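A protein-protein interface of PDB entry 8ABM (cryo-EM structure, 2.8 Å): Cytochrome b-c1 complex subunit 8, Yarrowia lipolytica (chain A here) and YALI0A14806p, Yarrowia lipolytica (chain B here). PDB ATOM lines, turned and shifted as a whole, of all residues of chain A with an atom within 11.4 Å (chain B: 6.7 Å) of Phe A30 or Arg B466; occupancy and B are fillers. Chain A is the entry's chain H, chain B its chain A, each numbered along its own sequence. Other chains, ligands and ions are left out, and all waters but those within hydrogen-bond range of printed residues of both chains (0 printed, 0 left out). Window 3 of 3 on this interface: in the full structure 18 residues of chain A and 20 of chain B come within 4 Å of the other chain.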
ATOM      1  N   THR A  26      15.771 -14.612  30.040  1.00  0.00           N
ATOM      2  CA  THR A  26      14.886 -14.851  28.918  1.00  0.00           C
ATOM      3  C   THR A  26      15.340 -14.064  27.702  1.00  0.00           C
ATOM      4  O   THR A  26      16.165 -13.178  27.810  1.00  0.00           O
ATOM      5  CB  THR A  26      13.434 -14.550  29.286  1.00  0.00           C
ATOM      6  OG1 THR A  26      12.695 -15.104  28.198  1.00  0.00           O
ATOM      7  CG2 THR A  26      13.151 -13.075  29.468  1.00  0.00           C
ATOM      8  N   ILE A  27      14.763 -14.370  26.550  1.00  0.00           N
ATOM      9  CA  ILE A  27      15.149 -13.660  25.345  1.00  0.00           C
ATOM     10  C   ILE A  27      13.949 -12.925  24.757  1.00  0.00           C
ATOM     11  O   ILE A  27      12.802 -13.262  25.040  1.00  0.00           O
ATOM     12  CB  ILE A  27      15.796 -14.630  24.350  1.00  0.00           C
ATOM     13  CG1 ILE A  27      14.819 -15.748  23.983  1.00  0.00           C
ATOM     14  CG2 ILE A  27      17.102 -15.165  24.924  1.00  0.00           C
ATOM     15  CD1 ILE A  27      15.231 -16.530  22.767  1.00  0.00           C
ATOM     16  N   SER A  28      14.239 -11.942  23.899  1.00  0.00           N
ATOM     17  CA  SER A  28      13.255 -11.081  23.263  1.00  0.00           C
ATOM     18  C   SER A  28      12.304 -11.903  22.405  1.00  0.00           C
ATOM     19  O   SER A  28      12.736 -12.869  21.789  1.00  0.00           O
ATOM     20  CB  SER A  28      13.963 -10.109  22.393  1.00  0.00           C
ATOM     21  OG  SER A  28      13.029  -9.337  21.670  1.00  0.00           O
ATOM     22  N   PRO A  29      11.011 -11.520  22.289  1.00  0.00           N
ATOM     23  CA  PRO A  29      10.095 -12.166  21.352  1.00  0.00           C
ATOM     24  C   PRO A  29      10.590 -12.069  19.917  1.00  0.00           C
ATOM     25  O   PRO A  29      10.361 -12.985  19.140  1.00  0.00           O
ATOM     26  CB  PRO A  29       8.776 -11.402  21.488  1.00  0.00           C
ATOM     27  CG  PRO A  29       9.162 -10.119  22.173  1.00  0.00           C
ATOM     28  CD  PRO A  29      10.348 -10.457  23.053  1.00  0.00           C
ATOM     29  N   PHE A  30      11.298 -10.988  19.584  1.00  0.00           N
ATOM     30  CA  PHE A  30      11.801 -10.855  18.228  1.00  0.00           C
ATOM     31  C   PHE A  30      13.034 -11.714  17.983  1.00  0.00           C
ATOM     32  O   PHE A  30      13.392 -11.943  16.834  1.00  0.00           O
ATOM     33  CB  PHE A  30      12.137  -9.404  17.912  1.00  0.00           C
ATOM     34  CG  PHE A  30      10.925  -8.522  17.815  1.00  0.00           C
ATOM     35  CD1 PHE A  30      10.311  -8.293  16.589  1.00  0.00           C
ATOM     36  CD2 PHE A  30      10.385  -7.930  18.953  1.00  0.00           C
ATOM     37  CE1 PHE A  30       9.187  -7.482  16.502  1.00  0.00           C
ATOM     38  CE2 PHE A  30       9.253  -7.126  18.867  1.00  0.00           C
ATOM     39  CZ  PHE A  30       8.661  -6.900  17.640  1.00  0.00           C
ATOM     40  N   ALA A  31      13.694 -12.170  19.047  1.00  0.00           N
ATOM     41  CA  ALA A  31      14.869 -13.002  18.854  1.00  0.00           C
ATOM     42  C   ALA A  31      14.499 -14.487  18.867  1.00  0.00           C
ATOM     43  O   ALA A  31      15.322 -15.335  18.533  1.00  0.00           O
ATOM     44  CB  ALA A  31      15.866 -12.678  19.927  1.00  0.00           C
ATOM     45  N   ALA A  32      13.269 -14.799  19.276  1.00  0.00           N
ATOM     46  CA  ALA A  32      12.882 -16.188  19.439  1.00  0.00           C
ATOM     47  C   ALA A  32      12.046 -16.662  18.259  1.00  0.00           C
ATOM     48  O   ALA A  32      11.359 -15.884  17.602  1.00  0.00           O
ATOM     49  CB  ALA A  32      12.117 -16.356  20.713  1.00  0.00           C
ATOM     50  N   ARG A  33      12.108 -17.971  18.012  1.00  0.00           N
ATOM     51  CA  ARG A  33      11.192 -18.590  17.078  1.00  0.00           C
ATOM     52  C   ARG A  33       9.942 -18.960  17.871  1.00  0.00           C
ATOM     53  O   ARG A  33       9.983 -19.853  18.712  1.00  0.00           O
ATOM     54  CB  ARG A  33      11.868 -19.782  16.403  1.00  0.00           C
ATOM     55  CG  ARG A  33      13.070 -19.428  15.539  1.00  0.00           C
ATOM     56  CD  ARG A  33      13.505 -20.504  14.563  1.00  0.00           C
ATOM     57  NE  ARG A  33      13.868 -21.747  15.230  1.00  0.00           N
ATOM     58  CZ  ARG A  33      15.094 -22.078  15.632  1.00  0.00           C
ATOM     59  NH1 ARG A  33      16.119 -21.264  15.434  1.00  0.00           N
ATOM     60  NH2 ARG A  33      15.292 -23.244  16.223  1.00  0.00           N
ATOM     61  N   PRO A  34       8.778 -18.318  17.633  1.00  0.00           N
ATOM     62  CA  PRO A  34       7.610 -18.526  18.486  1.00  0.00           C
ATOM     63  C   PRO A  34       7.083 -19.952  18.363  1.00  0.00           C
ATOM     64  O   PRO A  34       6.542 -20.499  19.322  1.00  0.00           O
ATOM     65  CB  PRO A  34       6.554 -17.548  17.958  1.00  0.00           C
ATOM     66  CG  PRO A  34       7.310 -16.640  17.016  1.00  0.00           C
ATOM     67  CD  PRO A  34       8.479 -17.447  16.492  1.00  0.00           C
ATOM     68  N   PHE A  35       7.311 -20.563  17.200  1.00  0.00           N
ATOM     69  CA  PHE A  35       6.811 -21.897  16.938  1.00  0.00           C
ATOM     70  C   PHE A  35       7.915 -22.939  16.979  1.00  0.00           C
ATOM     71  O   PHE A  35       7.767 -24.005  16.381  1.00  0.00           O
ATOM     72  CB  PHE A  35       6.145 -21.934  15.567  1.00  0.00           C
ATOM     73  CG  PHE A  35       4.769 -21.337  15.586  1.00  0.00           C
ATOM     74  CD1 PHE A  35       4.565 -19.999  15.286  1.00  0.00           C
ATOM     75  CD2 PHE A  35       3.672 -22.108  15.930  1.00  0.00           C
ATOM     76  CE1 PHE A  35       3.291 -19.448  15.322  1.00  0.00           C
ATOM     77  CE2 PHE A  35       2.397 -21.565  15.953  1.00  0.00           C
ATOM     78  CZ  PHE A  35       2.208 -20.233  15.653  1.00  0.00           C
ATOM     79  N   LEU B 367      12.530   5.336  29.198  1.00  0.00           N
ATOM     80  CA  LEU B 367      12.449   4.865  27.825  1.00  0.00           C
ATOM     81  C   LEU B 367      11.690   5.856  26.953  1.00  0.00           C
ATOM     82  O   LEU B 367      11.951   5.951  25.757  1.00  0.00           O
ATOM     83  CB  LEU B 367      11.853   3.462  27.765  1.00  0.00           C
ATOM     84  CG  LEU B 367      12.724   2.367  28.376  1.00  0.00           C
ATOM     85  CD1 LEU B 367      12.319   1.036  27.811  1.00  0.00           C
ATOM     86  CD2 LEU B 367      14.204   2.590  28.109  1.00  0.00           C
ATOM     87  N   TYR B 444      14.850   3.187  18.183  1.00  0.00           N
ATOM     88  CA  TYR B 444      13.405   3.163  18.079  1.00  0.00           C
ATOM     89  C   TYR B 444      12.930   1.744  17.815  1.00  0.00           C
ATOM     90  O   TYR B 444      13.361   1.132  16.840  1.00  0.00           O
ATOM     91  CB  TYR B 444      12.929   4.043  16.930  1.00  0.00           C
ATOM     92  CG  TYR B 444      11.480   4.351  17.134  1.00  0.00           C
ATOM     93  CD1 TYR B 444      11.107   5.206  18.159  1.00  0.00           C
ATOM     94  CD2 TYR B 444      10.488   3.724  16.393  1.00  0.00           C
ATOM     95  CE1 TYR B 444       9.778   5.493  18.416  1.00  0.00           C
ATOM     96  CE2 TYR B 444       9.150   3.995  16.640  1.00  0.00           C
ATOM     97  CZ  TYR B 444       8.798   4.871  17.660  1.00  0.00           C
ATOM     98  OH  TYR B 444       7.489   5.147  17.925  1.00  0.00           O
ATOM     99  N   ASP B 445      12.096   1.205  18.713  1.00  0.00           N
ATOM    100  CA  ASP B 445      11.512  -0.108  18.480  1.00  0.00           C
ATOM    101  C   ASP B 445      12.594  -1.181  18.308  1.00  0.00           C
ATOM    102  O   ASP B 445      12.470  -2.073  17.480  1.00  0.00           O
ATOM    103  CB  ASP B 445      10.585  -0.042  17.258  1.00  0.00           C
ATOM    104  CG  ASP B 445       9.730  -1.281  17.057  1.00  0.00           C
ATOM    105  OD1 ASP B 445       9.174  -1.777  18.062  1.00  0.00           O
ATOM    106  OD2 ASP B 445       9.625  -1.739  15.899  1.00  0.00           O
ATOM    107  N   LYS B 446      13.668  -1.122  19.092  1.00  0.00           N
ATOM    108  CA  LYS B 446      14.717  -2.118  18.963  1.00  0.00           C
ATOM    109  C   LYS B 446      14.738  -2.987  20.210  1.00  0.00           C
ATOM    110  O   LYS B 446      14.166  -2.613  21.224  1.00  0.00           O
ATOM    111  CB  LYS B 446      16.075  -1.449  18.780  1.00  0.00           C
ATOM    112  CG  LYS B 446      16.241  -0.725  17.458  1.00  0.00           C
ATOM    113  CD  LYS B 446      16.380  -1.671  16.294  1.00  0.00           C
ATOM    114  CE  LYS B 446      17.827  -1.979  15.971  1.00  0.00           C
ATOM    115  NZ  LYS B 446      17.935  -2.918  14.831  1.00  0.00           N
ATOM    116  N   ASP B 447      15.397  -4.144  20.117  1.00  0.00           N
ATOM    117  CA  ASP B 447      15.483  -5.049  21.245  1.00  0.00           C
ATOM    118  C   ASP B 447      16.482  -4.499  22.245  1.00  0.00           C
ATOM    119  O   ASP B 447      17.476  -3.883  21.863  1.00  0.00           O
ATOM    120  CB  ASP B 447      16.040  -6.394  20.809  1.00  0.00           C
ATOM    121  CG  ASP B 447      14.963  -7.367  20.388  1.00  0.00           C
ATOM    122  OD1 ASP B 447      13.771  -7.070  20.638  1.00  0.00           O
ATOM    123  OD2 ASP B 447      15.332  -8.428  19.829  1.00  0.00           O
ATOM    124  N   ILE B 448      16.210  -4.728  23.520  1.00  0.00           N
ATOM    125  CA  ILE B 448      17.103  -4.200  24.521  1.00  0.00           C
ATOM    126  C   ILE B 448      17.709  -5.377  25.255  1.00  0.00           C
ATOM    127  O   ILE B 448      17.161  -6.466  25.259  1.00  0.00           O
ATOM    128  CB  ILE B 448      16.304  -3.311  25.473  1.00  0.00           C
ATOM    129  CG1 ILE B 448      15.055  -4.055  25.928  1.00  0.00           C
ATOM    130  CG2 ILE B 448      15.939  -2.016  24.789  1.00  0.00           C
ATOM    131  CD1 ILE B 448      14.236  -3.265  26.883  1.00  0.00           C
ATOM    132  N   ASP B 461       7.941  -7.326  33.207  1.00  0.00           N
ATOM    133  CA  ASP B 461       8.522  -8.318  32.317  1.00  0.00           C
ATOM    134  C   ASP B 461       9.100  -7.676  31.051  1.00  0.00           C
ATOM    135  O   ASP B 461       8.850  -6.507  30.738  1.00  0.00           O
ATOM    136  CB  ASP B 461       7.439  -9.335  31.967  1.00  0.00           C
ATOM    137  CG  ASP B 461       6.130  -8.629  31.650  1.00  0.00           C
ATOM    138  OD1 ASP B 461       6.124  -7.854  30.684  1.00  0.00           O
ATOM    139  OD2 ASP B 461       5.136  -8.828  32.399  1.00  0.00           O
ATOM    140  N   TYR B 462       9.849  -8.482  30.297  1.00  0.00           N
ATOM    141  CA  TYR B 462      10.529  -7.989  29.115  1.00  0.00           C
ATOM    142  C   TYR B 462       9.590  -7.247  28.170  1.00  0.00           C
ATOM    143  O   TYR B 462       9.963  -6.177  27.711  1.00  0.00           O
ATOM    144  CB  TYR B 462      11.249  -9.108  28.371  1.00  0.00           C
ATOM    145  CG  TYR B 462      12.156  -8.591  27.292  1.00  0.00           C
ATOM    146  CD1 TYR B 462      13.480  -8.270  27.569  1.00  0.00           C
ATOM    147  CD2 TYR B 462      11.690  -8.411  25.995  1.00  0.00           C
ATOM    148  CE1 TYR B 462      14.318  -7.790  26.568  1.00  0.00           C
ATOM    149  CE2 TYR B 462      12.520  -7.932  24.989  1.00  0.00           C
ATOM    150  CZ  TYR B 462      13.842  -7.618  25.272  1.00  0.00           C
ATOM    151  OH  TYR B 462      14.654  -7.140  24.276  1.00  0.00           O
ATOM    152  N   ASN B 463       8.423  -7.816  27.840  1.00  0.00           N
ATOM    153  CA  ASN B 463       7.564  -7.196  26.841  1.00  0.00           C
ATOM    154  C   ASN B 463       7.172  -5.778  27.220  1.00  0.00           C
ATOM    155  O   ASN B 463       7.285  -4.861  26.415  1.00  0.00           O
ATOM    156  CB  ASN B 463       6.281  -7.969  26.582  1.00  0.00           C
ATOM    157  CG  ASN B 463       6.547  -9.092  25.617  1.00  0.00           C
ATOM    158  OD1 ASN B 463       7.106  -8.871  24.547  1.00  0.00           O
ATOM    159  ND2 ASN B 463       6.188 -10.296  26.011  1.00  0.00           N
ATOM    160  N   ARG B 464       6.765  -5.578  28.466  1.00  0.00           N
ATOM    161  CA  ARG B 464       6.329  -4.242  28.818  1.00  0.00           C
ATOM    162  C   ARG B 464       7.479  -3.244  28.772  1.00  0.00           C
ATOM    163  O   ARG B 464       7.245  -2.090  28.429  1.00  0.00           O
ATOM    164  CB  ARG B 464       5.587  -4.241  30.148  1.00  0.00           C
ATOM    165  CG  ARG B 464       4.203  -4.833  29.980  1.00  0.00           C
ATOM    166  CD  ARG B 464       3.395  -4.568  31.214  1.00  0.00           C
ATOM    167  NE  ARG B 464       2.977  -3.185  31.260  1.00  0.00           N
ATOM    168  CZ  ARG B 464       2.320  -2.660  32.281  1.00  0.00           C
ATOM    169  NH1 ARG B 464       2.002  -3.409  33.325  1.00  0.00           N
ATOM    170  NH2 ARG B 464       1.994  -1.383  32.261  1.00  0.00           N
ATOM    171  N   ILE B 465       8.695  -3.676  29.116  1.00  0.00           N
ATOM    172  CA  ILE B 465       9.811  -2.756  29.002  1.00  0.00           C
ATOM    173  C   ILE B 465      10.045  -2.483  27.521  1.00  0.00           C
ATOM    174  O   ILE B 465      10.114  -1.342  27.102  1.00  0.00           O
ATOM    175  CB  ILE B 465      11.094  -3.268  29.690  1.00  0.00           C
ATOM    176  CG1 ILE B 465      10.959  -3.648  31.171  1.00  0.00           C
ATOM    177  CG2 ILE B 465      12.231  -2.291  29.479  1.00  0.00           C
ATOM    178  CD1 ILE B 465       9.963  -2.868  31.981  1.00  0.00           C
ATOM    179  N   ARG B 466      10.168  -3.536  26.727  1.00  0.00           N
ATOM    180  CA  ARG B 466      10.426  -3.353  25.317  1.00  0.00           C
ATOM    181  C   ARG B 466       9.319  -2.573  24.608  1.00  0.00           C
ATOM    182  O   ARG B 466       9.585  -1.947  23.597  1.00  0.00           O
ATOM    183  CB  ARG B 466      10.547  -4.713  24.645  1.00  0.00           C
ATOM    184  CG  ARG B 466      11.360  -4.632  23.368  1.00  0.00           C
ATOM    185  CD  ARG B 466      10.532  -5.179  22.243  1.00  0.00           C
ATOM    186  NE  ARG B 466      11.388  -5.277  21.073  1.00  0.00           N
ATOM    187  CZ  ARG B 466      11.308  -4.462  20.029  1.00  0.00           C
ATOM    188  NH1 ARG B 466      10.404  -3.497  20.032  1.00  0.00           N
ATOM    189  NH2 ARG B 466      12.100  -4.640  18.984  1.00  0.00           N
ATOM    190  N   ASN B 467       8.073  -2.619  25.092  1.00  0.00           N
ATOM    191  CA  ASN B 467       7.020  -1.851  24.443  1.00  0.00           C
ATOM    192  C   ASN B 467       7.234  -0.353  24.585  1.00  0.00           C
ATOM    193  O   ASN B 467       6.721   0.417  23.777  1.00  0.00           O
ATOM    194  CB  ASN B 467       5.640  -2.144  25.009  1.00  0.00           C
ATOM    195  CG  ASN B 467       5.191  -3.531  24.629  1.00  0.00           C
ATOM    196  OD1 ASN B 467       5.755  -4.138  23.716  1.00  0.00           O
ATOM    197  ND2 ASN B 467       4.208  -4.050  25.348  1.00  0.00           N
ATOM    198  N   ASP B 468       7.976   0.066  25.613  1.00  0.00           N
ATOM    199  CA  ASP B 468       8.285   1.478  25.748  1.00  0.00           C
ATOM    200  C   ASP B 468       9.366   1.934  24.775  1.00  0.00           C
ATOM    201  O   ASP B 468       9.729   3.106  24.774  1.00  0.00           O
ATOM    202  CB  ASP B 468       8.621   1.833  27.191  1.00  0.00           C
ATOM    203  CG  ASP B 468       7.372   2.025  28.027  1.00  0.00           C
ATOM    204  OD1 ASP B 468       6.295   2.245  27.424  1.00  0.00           O
ATOM    205  OD2 ASP B 468       7.475   1.947  29.269  1.00  0.00           O
ATOM    206  N   MET B 469       9.876   1.032  23.936  1.00  0.00           N
ATOM    207  CA  MET B 469      10.880   1.461  22.982  1.00  0.00           C
ATOM    208  C   MET B 469      10.223   2.100  21.765  1.00  0.00           C
ATOM    209  O   MET B 469      10.921   2.461  20.821  1.00  0.00           O
ATOM    210  CB  MET B 469      11.768   0.306  22.520  1.00  0.00           C
ATOM    211  CG  MET B 469      12.638  -0.257  23.625  1.00  0.00           C
ATOM    212  SD  MET B 469      13.735   0.964  24.357  1.00  0.00           S
ATOM    213  CE  MET B 469      15.003   1.034  23.090  1.00  0.00           C
ATOM    214  N   SER B 470       8.894   2.222  21.770  1.00  0.00           N
ATOM    215  CA  SER B 470       8.254   2.986  20.710  1.00  0.00           C
ATOM    216  C   SER B 470       7.082   3.756  21.294  1.00  0.00           C
ATOM    217  O   SER B 470       6.705   3.516  22.435  1.00  0.00           O
ATOM    218  CB  SER B 470       7.824   2.101  19.578  1.00  0.00           C
ATOM    219  OG  SER B 470       6.935   1.107  20.066  1.00  0.00           O
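The side-chain carboxylate (OD1) of Asp B447 lies within hydrogen-bond range of the side-chain hydroxyl (OG) of Ser A28, at 2.6 Å.
O of Asn B463 sits close to OD1 of Asn B467.
The backbone carbonyl oxygen of Ile B448 sits at hydrogen-bond distance from the side-chain hydroxyl of Tyr B462, 2.8 Å away.
OG of Ser A28 lies close to N of Phe A30 (3.2 Å).
The guanidinium group of Arg B466 is in salt-bridge range of the side-chain carboxylate of Asp B445 (2.9 Å).
The guanidinium group of Arg B466 lies within salt-bridge range of the side-chain carboxylate of Asp B447, 3.0 Å away.
Among the printed residues, merely in contact across the chains: Pro A29 with Asn B463, Phe A30 with Arg B466, Ser A28 with Tyr B462, Pro A29 with Tyr B462 and Phe A30 with Asp B447.
Arg B466 touches just one residue of chain A: Phe A30.
No residue of chain A comes within 4 Å of Asp B445.
Printed residues of chain A within 4 Å of Asp B447: Ser A28 and Phe A30.
No residue of chain A comes within 4 Å of Ile B448.
Tyr B462 touches just these residues of chain A: Ser A28 (3.6 Å) and Pro A29 (3.8 Å).
Of chain A, only Pro A29 (3.4 Å) comes within 4 Å of Asn B463.
No residue of chain A comes within 4 Å of Asn B467.
Asp B468 touches none of the printed residues of chain A.
Met B469 touches none of the printed residues of chain A.
Of the printed residues of chain B, Pro A29 touches Tyr B462 (3.8 Å) and Asn B463 (3.4 Å).
Of the printed residues of chain B, Ser A28 touches Asp B447 (2.6 Å) and Tyr B462 (3.6 Å).
The nearest residue of chain A that does not touch Arg B466 is Ser A28 (4.4 Å).
Printed residues of chain B that touch a printed residue of chain A: Asp B447, Tyr B462, Asn B463 and Arg B466.
Of the 10 printed residues of chain A, 3 touch a printed residue of chain B.
Hydrophobic or aromatic side chains of chain A that line the printed part of chain B: Pro A29 and Phe A30.
Along chain A the printed residues that touch a printed residue of chain B span positions 28 to 30.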
